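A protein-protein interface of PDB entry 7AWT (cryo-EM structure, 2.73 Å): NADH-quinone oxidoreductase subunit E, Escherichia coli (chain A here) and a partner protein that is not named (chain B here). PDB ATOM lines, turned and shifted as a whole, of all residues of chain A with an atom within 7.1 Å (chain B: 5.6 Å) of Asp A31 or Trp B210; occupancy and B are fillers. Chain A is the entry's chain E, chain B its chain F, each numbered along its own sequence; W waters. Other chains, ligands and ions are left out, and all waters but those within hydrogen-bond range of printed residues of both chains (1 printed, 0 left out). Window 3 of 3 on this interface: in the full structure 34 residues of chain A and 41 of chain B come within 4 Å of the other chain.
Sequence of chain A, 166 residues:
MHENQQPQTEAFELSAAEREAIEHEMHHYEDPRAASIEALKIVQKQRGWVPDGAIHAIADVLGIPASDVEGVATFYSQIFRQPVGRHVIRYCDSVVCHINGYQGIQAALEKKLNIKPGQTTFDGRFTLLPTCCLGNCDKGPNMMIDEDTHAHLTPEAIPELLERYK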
ATOM      1  N   GLU A  25      -7.667   9.734  14.630  1.00  0.00           N
ATOM      2  CA  GLU A  25      -6.798   8.562  14.600  1.00  0.00           C
ATOM      3  C   GLU A  25      -7.393   7.401  15.379  1.00  0.00           C
ATOM      4  O   GLU A  25      -7.117   6.239  15.067  1.00  0.00           O
ATOM      5  CB  GLU A  25      -5.427   8.920  15.167  1.00  0.00           C
ATOM      6  CG  GLU A  25      -4.421   7.797  15.120  1.00  0.00           C
ATOM      7  CD  GLU A  25      -4.069   7.405  13.705  1.00  0.00           C
ATOM      8  OE1 GLU A  25      -4.413   8.160  12.772  1.00  0.00           O
ATOM      9  OE2 GLU A  25      -3.442   6.342  13.525  1.00  0.00           O
ATOM     10  N   MET A  26      -8.203   7.693  16.396  1.00  0.00           N
ATOM     11  CA  MET A  26      -8.724   6.646  17.268  1.00  0.00           C
ATOM     12  C   MET A  26      -9.681   5.692  16.570  1.00  0.00           C
ATOM     13  O   MET A  26      -9.958   4.621  17.119  1.00  0.00           O
ATOM     14  CB  MET A  26      -9.424   7.268  18.475  1.00  0.00           C
ATOM     15  CG  MET A  26      -8.494   7.628  19.613  1.00  0.00           C
ATOM     16  SD  MET A  26      -9.286   8.712  20.805  1.00  0.00           S
ATOM     17  CE  MET A  26     -10.827   7.844  21.060  1.00  0.00           C
ATOM     18  N   HIS A  27     -10.196   6.035  15.387  1.00  0.00           N
ATOM     19  CA  HIS A  27     -11.111   5.152  14.675  1.00  0.00           C
ATOM     20  C   HIS A  27     -10.474   4.525  13.441  1.00  0.00           C
ATOM     21  O   HIS A  27     -11.185   4.029  12.563  1.00  0.00           O
ATOM     22  CB  HIS A  27     -12.402   5.887  14.307  1.00  0.00           C
ATOM     23  CG  HIS A  27     -12.210   7.044  13.376  1.00  0.00           C
ATOM     24  ND1 HIS A  27     -11.644   6.904  12.127  1.00  0.00           N
ATOM     25  CD2 HIS A  27     -12.480   8.363  13.521  1.00  0.00           C
ATOM     26  CE1 HIS A  27     -11.588   8.085  11.537  1.00  0.00           C
ATOM     27  NE2 HIS A  27     -12.089   8.986  12.360  1.00  0.00           N
ATOM     28  N   HIS A  28      -9.146   4.541  13.356  1.00  0.00           N
ATOM     29  CA  HIS A  28      -8.436   3.712  12.393  1.00  0.00           C
ATOM     30  C   HIS A  28      -8.171   2.312  12.923  1.00  0.00           C
ATOM     31  O   HIS A  28      -7.699   1.460  12.167  1.00  0.00           O
ATOM     32  CB  HIS A  28      -7.103   4.354  12.012  1.00  0.00           C
ATOM     33  CG  HIS A  28      -7.238   5.549  11.124  1.00  0.00           C
ATOM     34  ND1 HIS A  28      -6.161   6.328  10.763  1.00  0.00           N
ATOM     35  CD2 HIS A  28      -8.319   6.097  10.523  1.00  0.00           C
ATOM     36  CE1 HIS A  28      -6.574   7.307   9.978  1.00  0.00           C
ATOM     37  NE2 HIS A  28      -7.879   7.189   9.817  1.00  0.00           N
ATOM     38  N   TYR A  29      -8.455   2.062  14.198  1.00  0.00           N
ATOM     39  CA  TYR A  29      -8.109   0.817  14.856  1.00  0.00           C
ATOM     40  C   TYR A  29      -9.334   0.244  15.549  1.00  0.00           C
ATOM     41  O   TYR A  29     -10.361   0.905  15.703  1.00  0.00           O
ATOM     42  CB  TYR A  29      -6.985   1.020  15.876  1.00  0.00           C
ATOM     43  CG  TYR A  29      -5.768   1.724  15.336  1.00  0.00           C
ATOM     44  CD1 TYR A  29      -4.743   1.013  14.737  1.00  0.00           C
ATOM     45  CD2 TYR A  29      -5.635   3.095  15.441  1.00  0.00           C
ATOM     46  CE1 TYR A  29      -3.627   1.648  14.252  1.00  0.00           C
ATOM     47  CE2 TYR A  29      -4.524   3.740  14.956  1.00  0.00           C
ATOM     48  CZ  TYR A  29      -3.523   3.013  14.363  1.00  0.00           C
ATOM     49  OH  TYR A  29      -2.410   3.653  13.878  1.00  0.00           O
ATOM     50  N   GLU A  30      -9.206  -1.011  15.974  1.00  0.00           N
ATOM     51  CA  GLU A  30     -10.275  -1.666  16.714  1.00  0.00           C
ATOM     52  C   GLU A  30     -10.271  -1.262  18.183  1.00  0.00           C
ATOM     53  O   GLU A  30     -11.330  -1.226  18.816  1.00  0.00           O
ATOM     54  CB  GLU A  30     -10.137  -3.182  16.566  1.00  0.00           C
ATOM     55  CG  GLU A  30     -10.897  -4.006  17.578  1.00  0.00           C
ATOM     56  CD  GLU A  30     -10.573  -5.479  17.474  1.00  0.00           C
ATOM     57  OE1 GLU A  30     -10.257  -5.936  16.357  1.00  0.00           O
ATOM     58  OE2 GLU A  30     -10.628  -6.178  18.506  1.00  0.00           O
ATOM     59  N   ASP A  31      -9.104  -0.933  18.728  1.00  0.00           N
ATOM     60  CA  ASP A  31      -8.950  -0.515  20.107  1.00  0.00           C
ATOM     61  C   ASP A  31      -8.455   0.924  20.148  1.00  0.00           C
ATOM     62  O   ASP A  31      -7.494   1.260  19.443  1.00  0.00           O
ATOM     63  CB  ASP A  31      -7.957  -1.432  20.836  1.00  0.00           C
ATOM     64  CG  ASP A  31      -8.116  -1.394  22.340  1.00  0.00           C
ATOM     65  OD1 ASP A  31      -8.130  -0.289  22.918  1.00  0.00           O
ATOM     66  OD2 ASP A  31      -8.216  -2.477  22.950  1.00  0.00           O
ATOM     67  N   PRO A  32      -9.081   1.803  20.933  1.00  0.00           N
ATOM     68  CA  PRO A  32      -8.577   3.181  21.031  1.00  0.00           C
ATOM     69  C   PRO A  32      -7.139   3.265  21.501  1.00  0.00           C
ATOM     70  O   PRO A  32      -6.432   4.208  21.132  1.00  0.00           O
ATOM     71  CB  PRO A  32      -9.532   3.832  22.038  1.00  0.00           C
ATOM     72  CG  PRO A  32     -10.771   3.032  21.952  1.00  0.00           C
ATOM     73  CD  PRO A  32     -10.346   1.625  21.664  1.00  0.00           C
ATOM     74  N   ARG A  33      -6.674   2.273  22.220  1.00  0.00           N
ATOM     75  CA  ARG A  33      -5.351   2.346  22.766  1.00  0.00           C
ATOM     76  C   ARG A  33      -4.371   2.460  21.635  1.00  0.00           C
ATOM     77  O   ARG A  33      -3.353   3.091  21.777  1.00  0.00           O
ATOM     78  CB  ARG A  33      -5.058   1.114  23.566  1.00  0.00           C
ATOM     79  CG  ARG A  33      -3.599   0.934  23.852  1.00  0.00           C
ATOM     80  CD  ARG A  33      -3.370  -0.441  24.412  1.00  0.00           C
ATOM     81  NE  ARG A  33      -4.050  -0.588  25.677  1.00  0.00           N
ATOM     82  CZ  ARG A  33      -3.499  -0.256  26.823  1.00  0.00           C
ATOM     83  NH1 ARG A  33      -2.274   0.225  26.829  1.00  0.00           N
ATOM     84  NH2 ARG A  33      -4.165  -0.402  27.946  1.00  0.00           N
ATOM     85  N   ALA A  34      -4.645   1.796  20.523  1.00  0.00           N
ATOM     86  CA  ALA A  34      -3.687   1.677  19.432  1.00  0.00           C
ATOM     87  C   ALA A  34      -3.248   3.025  18.886  1.00  0.00           C
ATOM     88  O   ALA A  34      -2.212   3.098  18.218  1.00  0.00           O
ATOM     89  CB  ALA A  34      -4.276   0.832  18.309  1.00  0.00           C
ATOM     90  N   ALA A  35      -4.001   4.085  19.151  1.00  0.00           N
ATOM     91  CA  ALA A  35      -3.641   5.416  18.688  1.00  0.00           C
ATOM     92  C   ALA A  35      -2.696   6.137  19.634  1.00  0.00           C
ATOM     93  O   ALA A  35      -2.531   7.350  19.504  1.00  0.00           O
ATOM     94  CB  ALA A  35      -4.899   6.259  18.480  1.00  0.00           C
ATOM     95  N   SER A  36      -2.055   5.424  20.562  1.00  0.00           N
ATOM     96  CA  SER A  36      -1.250   6.084  21.584  1.00  0.00           C
ATOM     97  C   SER A  36       0.031   6.665  20.998  1.00  0.00           C
ATOM     98  O   SER A  36       0.389   7.815  21.282  1.00  0.00           O
ATOM     99  CB  SER A  36      -0.928   5.100  22.705  1.00  0.00           C
ATOM    100  OG  SER A  36      -0.131   4.037  22.227  1.00  0.00           O
ATOM    101  N   ILE A  64      -7.096   5.162  28.332  1.00  0.00           N
ATOM    102  CA  ILE A  64      -6.128   4.299  29.002  1.00  0.00           C
ATOM    103  C   ILE A  64      -5.464   5.122  30.100  1.00  0.00           C
ATOM    104  O   ILE A  64      -5.514   6.358  30.050  1.00  0.00           O
ATOM    105  CB  ILE A  64      -5.110   3.737  27.999  1.00  0.00           C
ATOM    106  CG1 ILE A  64      -4.191   4.840  27.491  1.00  0.00           C
ATOM    107  CG2 ILE A  64      -5.829   3.103  26.832  1.00  0.00           C
ATOM    108  CD1 ILE A  64      -3.289   4.400  26.370  1.00  0.00           C
ATOM    109  N   TYR B  86      -6.356  -9.763  10.080  1.00  0.00           N
ATOM    110  CA  TYR B  86      -5.494  -8.639   9.765  1.00  0.00           C
ATOM    111  C   TYR B  86      -4.265  -9.106   9.002  1.00  0.00           C
ATOM    112  O   TYR B  86      -3.762 -10.212   9.213  1.00  0.00           O
ATOM    113  CB  TYR B  86      -5.064  -7.902  11.038  1.00  0.00           C
ATOM    114  CG  TYR B  86      -6.208  -7.221  11.743  1.00  0.00           C
ATOM    115  CD1 TYR B  86      -6.783  -6.076  11.221  1.00  0.00           C
ATOM    116  CD2 TYR B  86      -6.724  -7.731  12.924  1.00  0.00           C
ATOM    117  CE1 TYR B  86      -7.831  -5.455  11.855  1.00  0.00           C
ATOM    118  CE2 TYR B  86      -7.774  -7.113  13.564  1.00  0.00           C
ATOM    119  CZ  TYR B  86      -8.324  -5.977  13.024  1.00  0.00           C
ATOM    120  OH  TYR B  86      -9.371  -5.356  13.658  1.00  0.00           O
ATOM    121  N   TYR B 129      -2.381  -3.021   7.671  1.00  0.00           N
ATOM    122  CA  TYR B 129      -1.608  -1.948   8.278  1.00  0.00           C
ATOM    123  C   TYR B 129      -0.180  -2.015   7.766  1.00  0.00           C
ATOM    124  O   TYR B 129       0.510  -3.016   7.977  1.00  0.00           O
ATOM    125  CB  TYR B 129      -1.636  -2.053   9.802  1.00  0.00           C
ATOM    126  CG  TYR B 129      -3.001  -1.838  10.397  1.00  0.00           C
ATOM    127  CD1 TYR B 129      -3.881  -2.892  10.559  1.00  0.00           C
ATOM    128  CD2 TYR B 129      -3.414  -0.578  10.790  1.00  0.00           C
ATOM    129  CE1 TYR B 129      -5.129  -2.698  11.099  1.00  0.00           C
ATOM    130  CE2 TYR B 129      -4.661  -0.376  11.329  1.00  0.00           C
ATOM    131  CZ  TYR B 129      -5.513  -1.439  11.482  1.00  0.00           C
ATOM    132  OH  TYR B 129      -6.758  -1.245  12.021  1.00  0.00           O
ATOM    133  N   ILE B 187       3.294  -6.538  16.415  1.00  0.00           N
ATOM    134  CA  ILE B 187       1.883  -6.617  16.771  1.00  0.00           C
ATOM    135  C   ILE B 187       1.612  -5.838  18.049  1.00  0.00           C
ATOM    136  O   ILE B 187       0.632  -5.088  18.143  1.00  0.00           O
ATOM    137  CB  ILE B 187       1.460  -8.089  16.902  1.00  0.00           C
ATOM    138  CG1 ILE B 187       1.531  -8.779  15.543  1.00  0.00           C
ATOM    139  CG2 ILE B 187       0.079  -8.186  17.477  1.00  0.00           C
ATOM    140  CD1 ILE B 187       1.298 -10.258  15.605  1.00  0.00           C
ATOM    141  N   LEU B 190       1.812  -2.134  17.279  1.00  0.00           N
ATOM    142  CA  LEU B 190       0.613  -1.703  16.570  1.00  0.00           C
ATOM    143  C   LEU B 190      -0.583  -1.619  17.505  1.00  0.00           C
ATOM    144  O   LEU B 190      -1.463  -0.777  17.309  1.00  0.00           O
ATOM    145  CB  LEU B 190       0.315  -2.654  15.413  1.00  0.00           C
ATOM    146  CG  LEU B 190      -0.882  -2.310  14.530  1.00  0.00           C
ATOM    147  CD1 LEU B 190      -0.442  -1.487  13.341  1.00  0.00           C
ATOM    148  CD2 LEU B 190      -1.586  -3.569  14.074  1.00  0.00           C
ATOM    149  N   GLU B 191      -0.631  -2.476  18.524  1.00  0.00           N
ATOM    150  CA  GLU B 191      -1.691  -2.390  19.519  1.00  0.00           C
ATOM    151  C   GLU B 191      -1.596  -1.143  20.382  1.00  0.00           C
ATOM    152  O   GLU B 191      -2.520  -0.878  21.156  1.00  0.00           O
ATOM    153  CB  GLU B 191      -1.667  -3.618  20.425  1.00  0.00           C
ATOM    154  CG  GLU B 191      -2.190  -4.885  19.801  1.00  0.00           C
ATOM    155  CD  GLU B 191      -2.654  -5.872  20.845  1.00  0.00           C
ATOM    156  OE1 GLU B 191      -3.443  -5.475  21.725  1.00  0.00           O
ATOM    157  OE2 GLU B 191      -2.223  -7.039  20.803  1.00  0.00           O
ATOM    158  N   ARG B 193       1.023  -0.583  22.599  1.00  0.00           N
ATOM    159  CA  ARG B 193       1.687  -0.943  23.838  1.00  0.00           C
ATOM    160  C   ARG B 193       3.198  -0.849  23.663  1.00  0.00           C
ATOM    161  O   ARG B 193       3.704  -0.471  22.604  1.00  0.00           O
ATOM    162  CB  ARG B 193       1.279  -2.349  24.274  1.00  0.00           C
ATOM    163  CG  ARG B 193      -0.202  -2.613  24.162  1.00  0.00           C
ATOM    164  CD  ARG B 193      -0.515  -4.079  24.337  1.00  0.00           C
ATOM    165  NE  ARG B 193      -1.950  -4.320  24.339  1.00  0.00           N
ATOM    166  CZ  ARG B 193      -2.704  -4.304  25.430  1.00  0.00           C
ATOM    167  NH1 ARG B 193      -4.004  -4.532  25.345  1.00  0.00           N
ATOM    168  NH2 ARG B 193      -2.155  -4.064  26.610  1.00  0.00           N
ATOM    169  N   GLY B 208      -3.480 -13.064  16.861  1.00  0.00           N
ATOM    170  CA  GLY B 208      -2.462 -12.104  16.487  1.00  0.00           C
ATOM    171  C   GLY B 208      -2.693 -10.680  16.948  1.00  0.00           C
ATOM    172  O   GLY B 208      -2.436 -10.348  18.107  1.00  0.00           O
ATOM    173  N   ALA B 209      -3.169  -9.832  16.035  1.00  0.00           N
ATOM    174  CA  ALA B 209      -3.211  -8.390  16.246  1.00  0.00           C
ATOM    175  C   ALA B 209      -3.998  -7.994  17.484  1.00  0.00           C
ATOM    176  O   ALA B 209      -3.429  -7.458  18.434  1.00  0.00           O
ATOM    177  CB  ALA B 209      -3.801  -7.697  15.021  1.00  0.00           C
ATOM    178  N   TRP B 210      -5.298  -8.248  17.491  1.00  0.00           N
ATOM    179  CA  TRP B 210      -6.157  -7.903  18.615  1.00  0.00           C
ATOM    180  C   TRP B 210      -6.893  -9.135  19.111  1.00  0.00           C
ATOM    181  O   TRP B 210      -8.091  -9.097  19.396  1.00  0.00           O
ATOM    182  CB  TRP B 210      -7.141  -6.801  18.231  1.00  0.00           C
ATOM    183  CG  TRP B 210      -6.551  -5.426  18.266  1.00  0.00           C
ATOM    184  CD1 TRP B 210      -6.424  -4.622  19.353  1.00  0.00           C
ATOM    185  CD2 TRP B 210      -6.015  -4.692  17.161  1.00  0.00           C
ATOM    186  NE1 TRP B 210      -5.836  -3.435  19.000  1.00  0.00           N
ATOM    187  CE2 TRP B 210      -5.576  -3.455  17.656  1.00  0.00           C
ATOM    188  CE3 TRP B 210      -5.861  -4.964  15.801  1.00  0.00           C
ATOM    189  CZ2 TRP B 210      -4.995  -2.492  16.842  1.00  0.00           C
ATOM    190  CZ3 TRP B 210      -5.282  -4.009  14.997  1.00  0.00           C
ATOM    191  CH2 TRP B 210      -4.859  -2.789  15.518  1.00  0.00           C
ATOM    192  N   GLY B 211      -6.177 -10.248  19.220  1.00  0.00           N
ATOM    193  CA  GLY B 211      -6.800 -11.528  19.454  1.00  0.00           C
ATOM    194  C   GLY B 211      -7.357 -12.180  18.214  1.00  0.00           C
ATOM    195  O   GLY B 211      -7.826 -13.321  18.289  1.00  0.00           O
ATOM    196  N   LYS B 212      -7.323 -11.493  17.083  1.00  0.00           N
ATOM    197  CA  LYS B 212      -7.784 -12.018  15.808  1.00  0.00           C
ATOM    198  C   LYS B 212      -6.623 -12.656  15.064  1.00  0.00           C
ATOM    199  O   LYS B 212      -5.461 -12.470  15.425  1.00  0.00           O
ATOM    200  CB  LYS B 212      -8.400 -10.885  14.992  1.00  0.00           C
ATOM    201  CG  LYS B 212      -9.271  -9.947  15.797  1.00  0.00           C
ATOM    202  CD  LYS B 212     -10.462 -10.669  16.387  1.00  0.00           C
ATOM    203  CE  LYS B 212     -11.413  -9.692  17.041  1.00  0.00           C
ATOM    204  NZ  LYS B 212     -10.717  -8.855  18.050  1.00  0.00           N
ATOM    205  N   THR B 214      -3.743 -13.135  12.254  1.00  0.00           N
ATOM    206  CA  THR B 214      -2.833 -12.122  11.739  1.00  0.00           C
ATOM    207  C   THR B 214      -1.606 -12.753  11.101  1.00  0.00           C
ATOM    208  O   THR B 214      -0.967 -13.619  11.701  1.00  0.00           O
ATOM    209  CB  THR B 214      -2.401 -11.173  12.858  1.00  0.00           C
ATOM    210  OG1 THR B 214      -3.473 -10.275  13.157  1.00  0.00           O
ATOM    211  CG2 THR B 214      -1.187 -10.372  12.445  1.00  0.00           C
HETATM  212  O   HOH W   1      -5.197  -2.621  21.738  1.00  0.00           O
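N of Ala A34 lies close to O of Glu B191 (3.5 Å). The backbone carbonyl oxygen of His A28 lies within hydrogen-bond range of the side-chain hydroxyl of Tyr B129, 2.9 Å away. OE1 of Glu A30 is in hydrogen-bond range of OH of Tyr B86 (2.9 Å). The side-chain amino group of Lys B212 is in salt-bridge range of the side-chain carboxylate of Glu A30.
O of Arg A33 sits close to OG of Ser A36 (3.4 Å). The backbone carbonyl oxygen (O) of Trp B210 sits at hydrogen-bond distance from the side-chain amino group (NZ) of Lys B212, 3.0 Å away. The backbone carbonyl oxygen of Ala B209 lies close to the side-chain carboxylate of Glu B191, at 2.7 Å. NE of Arg B193 is in salt-bridge range of OE1 of Glu B191 (3.2 Å). The side-chain carboxylate of Glu A25 sits at hydrogen-bond distance from a ring nitrogen (ND1) of His A28 (3.2 Å). OH of Tyr A29 sits at hydrogen-bond distance from OE2 of Glu A25, 2.9 Å away.
Water W1 lies within hydrogen-bond range of the indole nitrogen (NE1) of Trp B210, the backbone carbonyl oxygen (O) of Glu B191 and the side-chain carboxylate (OD2) of Asp A31.
Of chain B, only Trp B210 comes within 4 Å of Asp A31. Trp B210 touches four residues of chain A. No residue of chain A comes within 4 Å of Ala B209. Of the printed residues of chain B, Ala A34 touches Leu B190 (3.4 Å), Glu B191 (3.3 Å) and Trp B210 (3.7 Å). Printed residues of chain A within 4 Å of Leu B190: Ala A34. Printed residues of chain A within 4 Å of Arg B193: Arg A33 (3.8 Å). Glu A25 touches none of the printed residues of chain B. The nearest residue of chain A that does not touch Trp B210 is His A28 (6.1 Å). The nearest printed residue of chain B that does not touch Tyr A29 is Leu B190 (4.5 Å).
Printed residues of chain A that touch a printed residue of chain B: His A28, Tyr A29, Glu A30, Asp A31, Arg A33 and Ala A34. Hydrophobic or aromatic side chains of chain A that line the printed part of chain B: Tyr A29 and Ala A34. Along chain A the printed residues that touch a printed residue of chain B span positions 28 to 34. Of the 12 printed residues of chain B, 7 touch a printed residue of chain A. Among the printed residues, Asp or Glu carboxylates within 4 Å of a Lys or Arg side-chain nitrogen of the other chain: Glu A30 with Lys B212 (2.7 Å).
Among the printed residues, merely in contact across the chains: Ala A34 with Leu B190 (3.4 Å), Arg A33 with Glu B191 (3.4 Å), Asp A31 with Trp B210 (3.4 Å), Glu A30 with Trp B210 (3.6 Å), Tyr A29 with Tyr B129 (3.7 Å), Ala A34 with Trp B210 (3.7 Å), Arg A33 with Arg B193 (3.8 Å) and Tyr A29 with Trp B210 (3.9 Å).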
